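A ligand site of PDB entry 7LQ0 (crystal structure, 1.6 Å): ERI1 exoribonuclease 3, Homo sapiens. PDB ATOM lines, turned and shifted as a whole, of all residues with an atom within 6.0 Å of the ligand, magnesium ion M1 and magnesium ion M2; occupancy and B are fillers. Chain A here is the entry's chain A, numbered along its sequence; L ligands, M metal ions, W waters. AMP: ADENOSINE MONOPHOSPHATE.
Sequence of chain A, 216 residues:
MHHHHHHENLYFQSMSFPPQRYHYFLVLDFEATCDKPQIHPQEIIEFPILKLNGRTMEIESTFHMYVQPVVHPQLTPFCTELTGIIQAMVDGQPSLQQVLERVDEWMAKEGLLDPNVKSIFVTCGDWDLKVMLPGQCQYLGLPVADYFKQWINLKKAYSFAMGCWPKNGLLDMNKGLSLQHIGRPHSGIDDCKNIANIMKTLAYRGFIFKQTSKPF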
ATOM      1  N   ASP A  29       8.424  -6.461  11.030  1.00  0.00           N
ATOM      2  CA  ASP A  29       9.144  -6.639   9.766  1.00  0.00           C
ATOM      3  C   ASP A  29       8.753  -5.467   8.867  1.00  0.00           C
ATOM      4  O   ASP A  29       7.667  -5.480   8.285  1.00  0.00           O
ATOM      5  CB  ASP A  29       8.824  -7.990   9.143  1.00  0.00           C
ATOM      6  CG  ASP A  29       9.945  -8.510   8.209  1.00  0.00           C
ATOM      7  OD1 ASP A  29      10.268  -9.731   8.211  1.00  0.00           O
ATOM      8  OD2 ASP A  29      10.467  -7.732   7.429  1.00  0.00           O
ATOM      9  N   PHE A  30       9.589  -4.426   8.826  1.00  0.00           N
ATOM     10  CA  PHE A  30       9.277  -3.232   8.038  1.00  0.00           C
ATOM     11  C   PHE A  30       9.261  -3.526   6.546  1.00  0.00           C
ATOM     12  O   PHE A  30      10.014  -4.387   6.054  1.00  0.00           O
ATOM     13  CB  PHE A  30      10.316  -2.116   8.259  1.00  0.00           C
ATOM     14  CG  PHE A  30      10.357  -1.555   9.649  1.00  0.00           C
ATOM     15  CD1 PHE A  30       9.192  -1.119  10.296  1.00  0.00           C
ATOM     16  CD2 PHE A  30      11.585  -1.419  10.295  1.00  0.00           C
ATOM     17  CE1 PHE A  30       9.271  -0.579  11.592  1.00  0.00           C
ATOM     18  CE2 PHE A  30      11.643  -0.913  11.558  1.00  0.00           C
ATOM     19  CZ  PHE A  30      10.511  -0.429  12.197  1.00  0.00           C
ATOM     20  N   GLU A  31       8.473  -2.740   5.806  1.00  0.00           N
ATOM     21  CA  GLU A  31       8.847  -2.444   4.431  1.00  0.00           C
ATOM     22  C   GLU A  31       9.259  -0.986   4.327  1.00  0.00           C
ATOM     23  O   GLU A  31       8.831  -0.145   5.120  1.00  0.00           O
ATOM     24  CB  GLU A  31       7.701  -2.714   3.442  1.00  0.00           C
ATOM     25  CG  GLU A  31       7.172  -4.144   3.472  1.00  0.00           C
ATOM     26  CD  GLU A  31       8.242  -5.215   3.332  1.00  0.00           C
ATOM     27  OE1 GLU A  31       9.195  -5.076   2.522  1.00  0.00           O
ATOM     28  OE2 GLU A  31       8.109  -6.238   4.078  1.00  0.00           O
ATOM     29  N   ALA A  32      10.129  -0.677   3.347  1.00  0.00           N
ATOM     30  CA  ALA A  32      10.650   0.672   3.190  1.00  0.00           C
ATOM     31  C   ALA A  32      10.691   1.040   1.722  1.00  0.00           C
ATOM     32  O   ALA A  32      10.694   0.170   0.847  1.00  0.00           O
ATOM     33  CB  ALA A  32      12.110   0.827   3.759  1.00  0.00           C
ATOM     34  N   THR A  33      10.725   2.344   1.441  1.00  0.00           N
ATOM     35  CA  THR A  33      10.976   2.751   0.060  1.00  0.00           C
ATOM     36  C   THR A  33      12.278   2.108  -0.436  1.00  0.00           C
ATOM     37  O   THR A  33      13.189   1.800   0.343  1.00  0.00           O
ATOM     38  CB  THR A  33      11.114   4.280  -0.056  1.00  0.00           C
ATOM     39  OG1 THR A  33      12.144   4.723   0.844  1.00  0.00           O
ATOM     40  CG2 THR A  33       9.788   4.998   0.303  1.00  0.00           C
ATOM     41  N   CYS A  34      12.389   1.932  -1.747  1.00  0.00           N
ATOM     42  CA  CYS A  34      13.556   1.282  -2.330  1.00  0.00           C
ATOM     43  C   CYS A  34      13.512   1.573  -3.815  1.00  0.00           C
ATOM     44  O   CYS A  34      12.529   2.135  -4.315  1.00  0.00           O
ATOM     45  CB  CYS A  34      13.580  -0.233  -2.059  1.00  0.00           C
ATOM     46  SG  CYS A  34      11.957  -1.068  -2.437  1.00  0.00           S
ATOM     47  N   ASP A  35      14.582   1.149  -4.523  1.00  0.00           N
ATOM     48  CA  ASP A  35      14.744   1.379  -5.938  1.00  0.00           C
ATOM     49  C   ASP A  35      15.934   0.541  -6.383  1.00  0.00           C
ATOM     50  O   ASP A  35      16.628  -0.071  -5.551  1.00  0.00           O
ATOM     51  CB  ASP A  35      14.940   2.874  -6.281  1.00  0.00           C
ATOM     52  CG  ASP A  35      14.545   3.200  -7.737  1.00  0.00           C
ATOM     53  OD1 ASP A  35      14.162   2.250  -8.460  1.00  0.00           O
ATOM     54  OD2 ASP A  35      14.602   4.407  -8.143  1.00  0.00           O
ATOM     55  N   LYS A  36      16.177   0.530  -7.693  1.00  0.00           N
ATOM     56  CA  LYS A  36      17.349  -0.136  -8.249  1.00  0.00           C
ATOM     57  C   LYS A  36      18.133   0.904  -9.047  1.00  0.00           C
ATOM     58  O   LYS A  36      17.573   1.447 -10.024  1.00  0.00           O
ATOM     59  CB  LYS A  36      16.883  -1.282  -9.146  1.00  0.00           C
ATOM     60  CG  LYS A  36      17.546  -2.621  -8.957  1.00  0.00           C
ATOM     61  CD  LYS A  36      17.235  -3.159  -7.598  1.00  0.00           C
ATOM     62  CE  LYS A  36      17.682  -4.567  -7.418  1.00  0.00           C
ATOM     63  NZ  LYS A  36      17.749  -4.914  -5.989  1.00  0.00           N
ATOM     64  N   GLN A  38      19.813   1.346  -5.026  1.00  0.00           N
ATOM     65  CA  GLN A  38      18.975   1.596  -3.858  1.00  0.00           C
ATOM     66  C   GLN A  38      18.702   3.079  -3.678  1.00  0.00           C
ATOM     67  O   GLN A  38      19.572   3.943  -3.934  1.00  0.00           O
ATOM     68  CB  GLN A  38      19.626   1.019  -2.606  1.00  0.00           C
ATOM     69  CG  GLN A  38      18.733   1.049  -1.352  1.00  0.00           C
ATOM     70  CD  GLN A  38      17.421   0.313  -1.591  1.00  0.00           C
ATOM     71  OE1 GLN A  38      16.500   0.891  -2.184  1.00  0.00           O
ATOM     72  NE2 GLN A  38      17.340  -0.980  -1.205  1.00  0.00           N
ATOM     73  N   GLN A  42      16.328   5.573   2.560  1.00  0.00           N
ATOM     74  CA  GLN A  42      15.122   4.754   2.637  1.00  0.00           C
ATOM     75  C   GLN A  42      14.236   5.254   3.745  1.00  0.00           C
ATOM     76  O   GLN A  42      14.699   5.871   4.703  1.00  0.00           O
ATOM     77  CB  GLN A  42      15.462   3.295   2.913  1.00  0.00           C
ATOM     78  CG  GLN A  42      16.216   2.615   1.759  1.00  0.00           C
ATOM     79  CD  GLN A  42      16.387   1.141   2.027  1.00  0.00           C
ATOM     80  OE1 GLN A  42      17.400   0.718   2.587  1.00  0.00           O
ATOM     81  NE2 GLN A  42      15.377   0.353   1.642  1.00  0.00           N
ATOM     82  N   ILE A  45       7.643   2.457   5.105  1.00  0.00           N
ATOM     83  CA  ILE A  45       6.296   2.641   4.551  1.00  0.00           C
ATOM     84  C   ILE A  45       5.284   1.640   5.104  1.00  0.00           C
ATOM     85  O   ILE A  45       4.086   1.798   4.847  1.00  0.00           O
ATOM     86  CB  ILE A  45       6.290   2.579   2.995  1.00  0.00           C
ATOM     87  CG1 ILE A  45       6.825   1.208   2.509  1.00  0.00           C
ATOM     88  CG2 ILE A  45       7.145   3.720   2.408  1.00  0.00           C
ATOM     89  CD1 ILE A  45       6.849   1.088   0.977  1.00  0.00           C
ATOM     90  N   PHE A  78       9.802  -0.163  -8.782  1.00  0.00           N
ATOM     91  CA  PHE A  78      10.448  -1.277  -8.102  1.00  0.00           C
ATOM     92  C   PHE A  78       9.868  -1.517  -6.705  1.00  0.00           C
ATOM     93  O   PHE A  78       9.597  -2.649  -6.322  1.00  0.00           O
ATOM     94  CB  PHE A  78      11.968  -1.058  -8.012  1.00  0.00           C
ATOM     95  CG  PHE A  78      12.649  -2.165  -7.276  1.00  0.00           C
ATOM     96  CD1 PHE A  78      12.942  -3.373  -7.941  1.00  0.00           C
ATOM     97  CD2 PHE A  78      12.891  -2.066  -5.919  1.00  0.00           C
ATOM     98  CE1 PHE A  78      13.512  -4.424  -7.265  1.00  0.00           C
ATOM     99  CE2 PHE A  78      13.446  -3.130  -5.211  1.00  0.00           C
ATOM    100  CZ  PHE A  78      13.779  -4.321  -5.892  1.00  0.00           C
ATOM    101  N   LEU A  82       8.158  -4.933  -5.589  1.00  0.00           N
ATOM    102  CA  LEU A  82       8.722  -5.737  -4.515  1.00  0.00           C
ATOM    103  C   LEU A  82       7.704  -6.006  -3.393  1.00  0.00           C
ATOM    104  O   LEU A  82       7.554  -7.146  -2.934  1.00  0.00           O
ATOM    105  CB  LEU A  82       9.937  -5.040  -3.920  1.00  0.00           C
ATOM    106  CG  LEU A  82      10.643  -5.875  -2.840  1.00  0.00           C
ATOM    107  CD1 LEU A  82      11.383  -7.066  -3.503  1.00  0.00           C
ATOM    108  CD2 LEU A  82      11.601  -4.989  -1.969  1.00  0.00           C
ATOM    109  N   THR A  83       7.068  -4.949  -2.890  1.00  0.00           N
ATOM    110  CA  THR A  83       6.284  -5.013  -1.656  1.00  0.00           C
ATOM    111  C   THR A  83       4.799  -5.186  -1.881  1.00  0.00           C
ATOM    112  O   THR A  83       4.084  -5.544  -0.922  1.00  0.00           O
ATOM    113  CB  THR A  83       6.457  -3.742  -0.830  1.00  0.00           C
ATOM    114  OG1 THR A  83       5.898  -2.642  -1.571  1.00  0.00           O
ATOM    115  CG2 THR A  83       7.976  -3.492  -0.536  1.00  0.00           C
ATOM    116  N   CYS A 124      13.494 -10.553  11.562  1.00  0.00           N
ATOM    117  CA  CYS A 124      14.273 -11.423  10.700  1.00  0.00           C
ATOM    118  C   CYS A 124      15.480 -10.626  10.235  1.00  0.00           C
ATOM    119  O   CYS A 124      15.389  -9.839   9.296  1.00  0.00           O
ATOM    120  CB  CYS A 124      13.433 -11.891   9.516  1.00  0.00           C
ATOM    121  SG  CYS A 124      14.329 -13.052   8.442  1.00  0.00           S
ATOM    122  N   TRP A 127      18.424  -5.787  10.578  1.00  0.00           N
ATOM    123  CA  TRP A 127      18.337  -4.530   9.838  1.00  0.00           C
ATOM    124  C   TRP A 127      17.259  -3.604  10.410  1.00  0.00           C
ATOM    125  O   TRP A 127      17.447  -2.381  10.519  1.00  0.00           O
ATOM    126  CB  TRP A 127      18.067  -4.832   8.367  1.00  0.00           C
ATOM    127  CG  TRP A 127      17.893  -3.613   7.492  1.00  0.00           C
ATOM    128  CD1 TRP A 127      18.897  -2.781   6.983  1.00  0.00           C
ATOM    129  CD2 TRP A 127      16.663  -3.090   7.017  1.00  0.00           C
ATOM    130  NE1 TRP A 127      18.340  -1.789   6.212  1.00  0.00           N
ATOM    131  CE2 TRP A 127      16.968  -1.934   6.237  1.00  0.00           C
ATOM    132  CE3 TRP A 127      15.322  -3.482   7.158  1.00  0.00           C
ATOM    133  CZ2 TRP A 127      15.986  -1.205   5.581  1.00  0.00           C
ATOM    134  CZ3 TRP A 127      14.328  -2.713   6.521  1.00  0.00           C
ATOM    135  CH2 TRP A 127      14.676  -1.586   5.759  1.00  0.00           C
ATOM    136  N   ASP A 128      16.092  -4.158  10.713  1.00  0.00           N
ATOM    137  CA  ASP A 128      14.954  -3.301  11.058  1.00  0.00           C
ATOM    138  C   ASP A 128      15.241  -2.374  12.223  1.00  0.00           C
ATOM    139  O   ASP A 128      14.972  -1.160  12.147  1.00  0.00           O
ATOM    140  CB  ASP A 128      13.740  -4.180  11.395  1.00  0.00           C
ATOM    141  CG  ASP A 128      13.370  -5.068  10.254  1.00  0.00           C
ATOM    142  OD1 ASP A 128      12.313  -4.868   9.653  1.00  0.00           O
ATOM    143  OD2 ASP A 128      14.159  -5.982   9.942  1.00  0.00           O
ATOM    144  N   PRO A 185       5.776 -12.966   0.170  1.00  0.00           N
ATOM    145  CA  PRO A 185       7.073 -12.407   0.650  1.00  0.00           C
ATOM    146  C   PRO A 185       7.141 -10.901   0.420  1.00  0.00           C
ATOM    147  O   PRO A 185       6.615 -10.391  -0.570  1.00  0.00           O
ATOM    148  CB  PRO A 185       8.114 -13.150  -0.213  1.00  0.00           C
ATOM    149  CG  PRO A 185       7.381 -14.468  -0.535  1.00  0.00           C
ATOM    150  CD  PRO A 185       5.966 -14.111  -0.752  1.00  0.00           C
ATOM    151  N   HIS A 186       7.763 -10.190   1.351  1.00  0.00           N
ATOM    152  CA  HIS A 186       7.953  -8.735   1.273  1.00  0.00           C
ATOM    153  C   HIS A 186       6.676  -7.920   1.483  1.00  0.00           C
ATOM    154  O   HIS A 186       6.661  -6.702   1.208  1.00  0.00           O
ATOM    155  CB  HIS A 186       8.596  -8.340  -0.059  1.00  0.00           C
ATOM    156  CG  HIS A 186       9.841  -9.098  -0.346  1.00  0.00           C
ATOM    157  ND1 HIS A 186      11.006  -8.911   0.365  1.00  0.00           N
ATOM    158  CD2 HIS A 186      10.113 -10.061  -1.262  1.00  0.00           C
ATOM    159  CE1 HIS A 186      11.936  -9.719  -0.103  1.00  0.00           C
ATOM    160  NE2 HIS A 186      11.423 -10.426  -1.097  1.00  0.00           N
ATOM    161  N   SER A 187       5.598  -8.535   1.974  1.00  0.00           N
ATOM    162  CA  SER A 187       4.517  -7.826   2.632  1.00  0.00           C
ATOM    163  C   SER A 187       4.865  -7.863   4.109  1.00  0.00           C
ATOM    164  O   SER A 187       5.169  -8.935   4.630  1.00  0.00           O
ATOM    165  CB  SER A 187       3.169  -8.506   2.390  1.00  0.00           C
ATOM    166  OG  SER A 187       2.261  -8.079   3.397  1.00  0.00           O
ATOM    167  N   GLY A 188       4.902  -6.688   4.749  1.00  0.00           N
ATOM    168  CA  GLY A 188       5.398  -6.648   6.115  1.00  0.00           C
ATOM    169  C   GLY A 188       4.549  -7.502   7.034  1.00  0.00           C
ATOM    170  O   GLY A 188       5.066  -8.307   7.817  1.00  0.00           O
ATOM    171  N   ASP A 191       5.210 -11.176   6.251  1.00  0.00           N
ATOM    172  CA  ASP A 191       6.516 -11.574   6.774  1.00  0.00           C
ATOM    173  C   ASP A 191       6.405 -11.815   8.280  1.00  0.00           C
ATOM    174  O   ASP A 191       6.955 -12.798   8.795  1.00  0.00           O
ATOM    175  CB  ASP A 191       7.536 -10.491   6.483  1.00  0.00           C
ATOM    176  CG  ASP A 191       8.044 -10.509   5.033  1.00  0.00           C
ATOM    177  OD1 ASP A 191       7.733 -11.440   4.256  1.00  0.00           O
ATOM    178  OD2 ASP A 191       8.786  -9.559   4.674  1.00  0.00           O
HETATM  179  P   AMP L   1      12.029  -7.303   3.366  1.00  0.00           P
HETATM  180  O1P AMP L   1      11.599  -7.371   4.836  1.00  0.00           O
HETATM  181  O2P AMP L   1      10.788  -7.006   2.500  1.00  0.00           O
HETATM  182  O3P AMP L   1      12.730  -8.514   2.812  1.00  0.00           O
HETATM  183  O5' AMP L   1      12.989  -6.069   3.147  1.00  0.00           O
HETATM  184  C5' AMP L   1      12.833  -4.840   3.817  1.00  0.00           C
HETATM  185  C4' AMP L   1      13.083  -3.699   2.849  1.00  0.00           C
HETATM  186  O4' AMP L   1      14.408  -3.841   2.263  1.00  0.00           O
HETATM  187  C3' AMP L   1      12.158  -3.651   1.642  1.00  0.00           C
HETATM  188  O3' AMP L   1      10.898  -3.013   1.921  1.00  0.00           O
HETATM  189  C2' AMP L   1      12.994  -2.854   0.644  1.00  0.00           C
HETATM  190  O2' AMP L   1      12.981  -1.479   1.019  1.00  0.00           O
HETATM  191  C1' AMP L   1      14.401  -3.413   0.919  1.00  0.00           C
HETATM  192  N9  AMP L   1      14.697  -4.573   0.065  1.00  0.00           N
HETATM  193  C8  AMP L   1      14.342  -5.859   0.334  1.00  0.00           C
HETATM  194  N7  AMP L   1      14.714  -6.686  -0.704  1.00  0.00           N
HETATM  195  C5  AMP L   1      15.278  -5.881  -1.633  1.00  0.00           C
HETATM  196  C6  AMP L   1      15.877  -6.105  -2.953  1.00  0.00           C
HETATM  197  N6  AMP L   1      15.937  -7.367  -3.443  1.00  0.00           N
HETATM  198  N1  AMP L   1      16.322  -5.036  -3.622  1.00  0.00           N
HETATM  199  C2  AMP L   1      16.224  -3.781  -3.115  1.00  0.00           C
HETATM  200  N3  AMP L   1      15.699  -3.500  -1.905  1.00  0.00           N
HETATM  201  C4  AMP L   1      15.237  -4.518  -1.150  1.00  0.00           C
HETATM  202 MG    MG M   1      12.443  -7.664   6.660  1.00  0.00          MG
HETATM  203 MG    MG M   2       9.352  -7.503   5.268  1.00  0.00          MG
HETATM  204  O   HOH W   1      12.245  -5.604   7.074  1.00  0.00           O
HETATM  205  O   HOH W   2      14.880 -10.065   2.522  1.00  0.00           O
HETATM  206  O   HOH W   3      17.310  -2.276   2.210  1.00  0.00           O
HETATM  207  O   HOH W   4      13.537  -7.852   8.439  1.00  0.00           O
HETATM  208  O   HOH W   5      14.266  -7.510   5.678  1.00  0.00           O
HETATM  209  O   HOH W   6      11.219 -10.597   3.628  1.00  0.00           O
HETATM  210  O   HOH W   7      12.315  -9.708   6.525  1.00  0.00           O
HETATM  211  O   HOH W   8      14.928  -9.736  -1.882  1.00  0.00           O
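NZ of Lys 36 lies within hydrogen-bond range of N1 of the ligand. N of Ala 32 is in hydrogen-bond range of O3' of the ligand (2.8 Å). O of Ala 32 lies within hydrogen-bond range of O2' of the ligand, 2.8 Å away. ND1 of His 186 lies within hydrogen-bond range of O2P of the ligand (2.9 Å). O2' of the ligand lies within hydrogen-bond range of NE2 of Gln 42 (3.1 Å). A nitrogen (N3) of the ligand is in hydrogen-bond range of the side-chain amide nitrogen (NE2) of Gln 38 (3.1 Å). The backbone carbonyl oxygen (O) of Thr 33 lies within hydrogen-bond range of an oxygen (O2') of the ligand, at 3.4 Å. SG of Cys 34 lies close to O2' of the ligand (3.6 Å).
The backbone NH of Gly 188 sits close to the side-chain carboxylate of Glu 31. The backbone NH of Ile 45 sits at hydrogen-bond distance from the backbone carbonyl oxygen of Glu 31 (2.9 Å). OD1 of Asp 191 lies within hydrogen-bond range of N of His 186. SG of Cys 34 is in hydrogen-bond range of O of Ala 32 (3.7 Å). The backbone carbonyl oxygen of Thr 33 lies within hydrogen-bond range of the side-chain amide nitrogen of Gln 42. The side-chain amide oxygen of Gln 38 sits at hydrogen-bond distance from the backbone NH of Asp 35, at 3.0 Å. N of Phe 30 sits at hydrogen-bond distance from OD1 of Asp 128, 2.9 Å away.
O of Phe 30 touches O1P of the ligand, at 3.6 Å. CZ of Phe 78 touches N1 of the ligand (3.5 Å). CD2 of Leu 82 touches C2' of the ligand (3.7 Å). Thr 83 touches the ligand. Trp 127 touches the ligand. 15 residues have an atom within 4 Å of the ligand: Asp 29, Phe 30, Glu 31, Ala 32, Thr 33, Cys 34, Lys 36, Gln 38, Gln 42, Phe 78, Leu 82, Thr 83, Trp 127, His 186 and Asp 191. The nearest printed residue that does not touch the ligand is Asp 35 (4.5 Å).
Within 4 Å of magnesium ion M1: Asp 29. The nearest printed residue that does not touch magnesium ion M1 is Asp 128 (4.1 Å).
Merely in contact with magnesium ion M2: Phe 30. The nearest printed residue that does not touch magnesium ion M2 is Gly 188 (4.1 Å).
Magnesium ion M1 is bound by an oxygen (O1P) of the ligand (2.0 Å), water W7 (2.1 Å), water W5 (2.1 Å), water W4 (2.1 Å), water W1 (2.1 Å) and the side-chain carboxylate (OD2) of Asp 29 (2.1 Å). Magnesium ion M1 has six donor atoms within binding distance.
Magnesium ion M2 is bound by the side-chain carboxylate of Glu 31 (2.1 Å), the side-chain carboxylate of Asp 191 (2.2 Å), an oxygen (O1P) of the ligand (2.3 Å) and the side-chain carboxylate of Asp 29 (2.4 Å). Magnesium ion M2 has four donor atoms within binding distance.
Water W1 bridges OD1 of Asp 128 (2.7 Å) and O of Phe 30 (2.7 Å). Water W4 lies within hydrogen-bond range of OD2 of Asp 128 and O of Cys 124. Water W3 bridges OE1 of Gln 42 (3.0 Å) and O4' of the ligand (3.3 Å).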
